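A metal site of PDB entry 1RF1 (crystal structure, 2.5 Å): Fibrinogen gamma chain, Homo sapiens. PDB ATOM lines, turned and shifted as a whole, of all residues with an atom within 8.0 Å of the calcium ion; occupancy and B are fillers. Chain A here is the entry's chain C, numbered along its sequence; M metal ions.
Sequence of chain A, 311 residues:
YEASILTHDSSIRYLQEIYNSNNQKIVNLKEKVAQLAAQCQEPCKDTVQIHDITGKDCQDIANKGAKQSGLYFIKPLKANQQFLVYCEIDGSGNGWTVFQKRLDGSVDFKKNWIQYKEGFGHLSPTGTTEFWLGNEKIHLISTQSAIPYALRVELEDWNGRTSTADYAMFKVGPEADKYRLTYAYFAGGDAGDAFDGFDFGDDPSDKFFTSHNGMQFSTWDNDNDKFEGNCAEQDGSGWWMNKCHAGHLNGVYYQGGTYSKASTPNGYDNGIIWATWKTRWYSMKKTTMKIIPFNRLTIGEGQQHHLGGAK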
ATOM      1  N   SER A 218     -18.344  -0.538 -20.198  1.00  0.00           N
ATOM      2  CA  SER A 218     -18.558  -1.964 -20.467  1.00  0.00           C
ATOM      3  C   SER A 218     -18.507  -2.865 -19.249  1.00  0.00           C
ATOM      4  O   SER A 218     -17.730  -2.631 -18.317  1.00  0.00           O
ATOM      5  CB  SER A 218     -17.544  -2.456 -21.498  1.00  0.00           C
ATOM      6  OG  SER A 218     -17.782  -1.876 -22.764  1.00  0.00           O
ATOM      7  N   ASN A 222     -22.612  -6.650 -20.841  1.00  0.00           N
ATOM      8  CA  ASN A 222     -22.958  -5.553 -21.732  1.00  0.00           C
ATOM      9  C   ASN A 222     -21.699  -5.001 -22.390  1.00  0.00           C
ATOM     10  O   ASN A 222     -21.082  -4.058 -21.893  1.00  0.00           O
ATOM     11  CB  ASN A 222     -23.676  -4.447 -20.943  1.00  0.00           C
ATOM     12  CG  ASN A 222     -24.398  -3.463 -21.839  1.00  0.00           C
ATOM     13  OD1 ASN A 222     -25.403  -2.884 -21.441  1.00  0.00           O
ATOM     14  ND2 ASN A 222     -23.887  -3.268 -23.047  1.00  0.00           N
ATOM     15  N   ASP A 223     -21.319  -5.608 -23.521  1.00  0.00           N
ATOM     16  CA  ASP A 223     -20.117  -5.252 -24.284  1.00  0.00           C
ATOM     17  C   ASP A 223     -20.295  -4.031 -25.193  1.00  0.00           C
ATOM     18  O   ASP A 223     -21.171  -4.006 -26.064  1.00  0.00           O
ATOM     19  CB  ASP A 223     -19.666  -6.443 -25.134  1.00  0.00           C
ATOM     20  CG  ASP A 223     -18.292  -6.225 -25.776  1.00  0.00           C
ATOM     21  OD1 ASP A 223     -18.011  -5.104 -26.252  1.00  0.00           O
ATOM     22  OD2 ASP A 223     -17.493  -7.181 -25.817  1.00  0.00           O
ATOM     23  N   ASN A 224     -19.443  -3.037 -24.997  1.00  0.00           N
ATOM     24  CA  ASN A 224     -19.472  -1.818 -25.809  1.00  0.00           C
ATOM     25  C   ASN A 224     -18.035  -1.354 -26.079  1.00  0.00           C
ATOM     26  O   ASN A 224     -17.791  -0.170 -26.310  1.00  0.00           O
ATOM     27  CB  ASN A 224     -20.261  -0.715 -25.089  1.00  0.00           C
ATOM     28  CG  ASN A 224     -21.697  -1.112 -24.758  1.00  0.00           C
ATOM     29  OD1 ASN A 224     -21.980  -1.638 -23.676  1.00  0.00           O
ATOM     30  ND2 ASN A 224     -22.609  -0.866 -25.690  1.00  0.00           N
ATOM     31  N   ASP A 225     -17.093  -2.297 -26.046  1.00  0.00           N
ATOM     32  CA  ASP A 225     -15.690  -1.970 -26.293  1.00  0.00           C
ATOM     33  C   ASP A 225     -15.302  -2.069 -27.767  1.00  0.00           C
ATOM     34  O   ASP A 225     -16.039  -2.633 -28.581  1.00  0.00           O
ATOM     35  CB  ASP A 225     -14.780  -2.898 -25.474  1.00  0.00           C
ATOM     36  CG  ASP A 225     -14.907  -4.359 -25.887  1.00  0.00           C
ATOM     37  OD1 ASP A 225     -14.952  -4.641 -27.100  1.00  0.00           O
ATOM     38  OD2 ASP A 225     -14.954  -5.224 -24.975  1.00  0.00           O
ATOM     39  N   LYS A 226     -14.138  -1.522 -28.115  1.00  0.00           N
ATOM     40  CA  LYS A 226     -13.634  -1.524 -29.479  1.00  0.00           C
ATOM     41  C   LYS A 226     -12.789  -2.761 -29.763  1.00  0.00           C
ATOM     42  O   LYS A 226     -11.768  -2.690 -30.430  1.00  0.00           O
ATOM     43  CB  LYS A 226     -12.779  -0.284 -29.740  1.00  0.00           C
ATOM     44  CG  LYS A 226     -13.417   1.031 -29.331  1.00  0.00           C
ATOM     45  CD  LYS A 226     -14.681   1.330 -30.120  1.00  0.00           C
ATOM     46  CE  LYS A 226     -15.237   2.702 -29.740  1.00  0.00           C
ATOM     47  NZ  LYS A 226     -16.549   3.012 -30.386  1.00  0.00           N
ATOM     48  N   PHE A 227     -13.226  -3.908 -29.252  1.00  0.00           N
ATOM     49  CA  PHE A 227     -12.517  -5.172 -29.429  1.00  0.00           C
ATOM     50  C   PHE A 227     -13.563  -6.230 -29.787  1.00  0.00           C
ATOM     51  O   PHE A 227     -14.676  -6.214 -29.271  1.00  0.00           O
ATOM     52  CB  PHE A 227     -11.808  -5.517 -28.104  1.00  0.00           C
ATOM     53  CG  PHE A 227     -11.189  -6.882 -28.062  1.00  0.00           C
ATOM     54  CD1 PHE A 227     -10.332  -7.318 -29.073  1.00  0.00           C
ATOM     55  CD2 PHE A 227     -11.426  -7.724 -26.976  1.00  0.00           C
ATOM     56  CE1 PHE A 227      -9.721  -8.569 -28.986  1.00  0.00           C
ATOM     57  CE2 PHE A 227     -10.815  -8.974 -26.890  1.00  0.00           C
ATOM     58  CZ  PHE A 227      -9.967  -9.399 -27.899  1.00  0.00           C
ATOM     59  N   GLU A 228     -13.214  -7.144 -30.694  1.00  0.00           N
ATOM     60  CA  GLU A 228     -14.179  -8.170 -31.097  1.00  0.00           C
ATOM     61  C   GLU A 228     -14.489  -9.113 -29.936  1.00  0.00           C
ATOM     62  O   GLU A 228     -15.531  -9.748 -29.900  1.00  0.00           O
ATOM     63  CB  GLU A 228     -13.655  -8.955 -32.298  1.00  0.00           C
ATOM     64  CG  GLU A 228     -12.494  -9.878 -32.000  1.00  0.00           C
ATOM     65  CD  GLU A 228     -12.128 -10.760 -33.187  1.00  0.00           C
ATOM     66  OE1 GLU A 228     -11.272 -11.656 -33.030  1.00  0.00           O
ATOM     67  OE2 GLU A 228     -12.695 -10.553 -34.286  1.00  0.00           O
ATOM     68  N   GLY A 229     -13.567  -9.192 -28.982  1.00  0.00           N
ATOM     69  CA  GLY A 229     -13.784 -10.034 -27.824  1.00  0.00           C
ATOM     70  C   GLY A 229     -14.494  -9.200 -26.773  1.00  0.00           C
ATOM     71  O   GLY A 229     -15.138  -8.193 -27.109  1.00  0.00           O
ATOM     72  N   ASN A 230     -14.379  -9.595 -25.516  1.00  0.00           N
ATOM     73  CA  ASN A 230     -15.040  -8.841 -24.453  1.00  0.00           C
ATOM     74  C   ASN A 230     -14.080  -8.466 -23.331  1.00  0.00           C
ATOM     75  O   ASN A 230     -13.875  -9.245 -22.398  1.00  0.00           O
ATOM     76  CB  ASN A 230     -16.209  -9.645 -23.901  1.00  0.00           C
ATOM     77  CG  ASN A 230     -17.026  -8.873 -22.887  1.00  0.00           C
ATOM     78  OD1 ASN A 230     -18.222  -9.080 -22.759  1.00  0.00           O
ATOM     79  ND2 ASN A 230     -16.382  -7.968 -22.152  1.00  0.00           N
ATOM     80  N   CYS A 231     -13.521  -7.267 -23.414  1.00  0.00           N
ATOM     81  CA  CYS A 231     -12.575  -6.793 -22.405  1.00  0.00           C
ATOM     82  C   CYS A 231     -13.099  -6.966 -20.977  1.00  0.00           C
ATOM     83  O   CYS A 231     -12.493  -7.672 -20.178  1.00  0.00           O
ATOM     84  CB  CYS A 231     -12.226  -5.329 -22.637  1.00  0.00           C
ATOM     85  SG  CYS A 231     -11.376  -4.932 -24.208  1.00  0.00           S
ATOM     86  N   ALA A 232     -14.219  -6.322 -20.679  1.00  0.00           N
ATOM     87  CA  ALA A 232     -14.796  -6.394 -19.334  1.00  0.00           C
ATOM     88  C   ALA A 232     -14.885  -7.819 -18.810  1.00  0.00           C
ATOM     89  O   ALA A 232     -14.595  -8.071 -17.637  1.00  0.00           O
ATOM     90  CB  ALA A 232     -16.173  -5.750 -19.330  1.00  0.00           C
ATOM     91  N   MET A 241     -13.727   0.527 -21.501  1.00  0.00           N
ATOM     92  CA  MET A 241     -12.814  -0.261 -22.326  1.00  0.00           C
ATOM     93  C   MET A 241     -12.758   0.136 -23.796  1.00  0.00           C
ATOM     94  O   MET A 241     -13.766   0.500 -24.405  1.00  0.00           O
ATOM     95  CB  MET A 241     -13.195  -1.744 -22.247  1.00  0.00           C
ATOM     96  CG  MET A 241     -13.292  -2.293 -20.840  1.00  0.00           C
ATOM     97  SD  MET A 241     -11.700  -2.411 -20.023  1.00  0.00           S
ATOM     98  CE  MET A 241     -11.926  -3.930 -19.095  1.00  0.00           C
ATOM     99  N   ASN A 242     -11.547   0.047 -24.344  1.00  0.00           N
ATOM    100  CA  ASN A 242     -11.292   0.342 -25.763  1.00  0.00           C
ATOM    101  C   ASN A 242     -10.882  -0.996 -26.359  1.00  0.00           C
ATOM    102  O   ASN A 242     -11.723  -1.725 -26.878  1.00  0.00           O
ATOM    103  CB  ASN A 242     -10.145   1.359 -25.915  1.00  0.00           C
ATOM    104  CG  ASN A 242      -9.924   1.793 -27.363  1.00  0.00           C
ATOM    105  OD1 ASN A 242     -10.045   1.000 -28.284  1.00  0.00           O
ATOM    106  ND2 ASN A 242      -9.568   3.060 -27.553  1.00  0.00           N
ATOM    107  N   LYS A 243      -9.580  -1.320 -26.286  1.00  0.00           N
ATOM    108  CA  LYS A 243      -9.054  -2.594 -26.794  1.00  0.00           C
ATOM    109  C   LYS A 243      -7.632  -2.899 -26.332  1.00  0.00           C
ATOM    110  O   LYS A 243      -6.726  -3.037 -27.158  1.00  0.00           O
ATOM    111  CB  LYS A 243      -9.099  -2.638 -28.328  1.00  0.00           C
ATOM    112  CG  LYS A 243      -8.608  -3.968 -28.915  1.00  0.00           C
ATOM    113  CD  LYS A 243      -9.183  -4.269 -30.297  1.00  0.00           C
ATOM    114  CE  LYS A 243      -8.475  -3.515 -31.416  1.00  0.00           C
ATOM    115  NZ  LYS A 243      -7.113  -4.065 -31.668  1.00  0.00           N
HETATM  116 CA    CA M   1     -16.338  -6.206 -28.005  1.00  0.00          CA
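C of Glu 228 touches the calcium ion (3.9 Å).
Within 4 Å of the calcium ion: Asp 223, Asp 225, Phe 227, Glu 228 and Gly 229.
The nearest printed residue that does not touch the calcium ion is Asn 230 (4.6 Å).
The calcium ion is bound by O of Phe 227 (2.1 Å), OD1 of Asp 225 (2.3 Å), O of Gly 229 (2.5 Å), OD2 of Asp 223 (2.7 Å) and OD1 of Asp 223 (2.7 Å).
The calcium ion has five donor atoms within binding distance.
The backbone NH of Asp 225 is in hydrogen-bond range of the side-chain hydroxyl of Ser 218, at 3.4 Å.
OD2 of Asp 225 lies within hydrogen-bond range of N of Cys 231 (2.9 Å).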
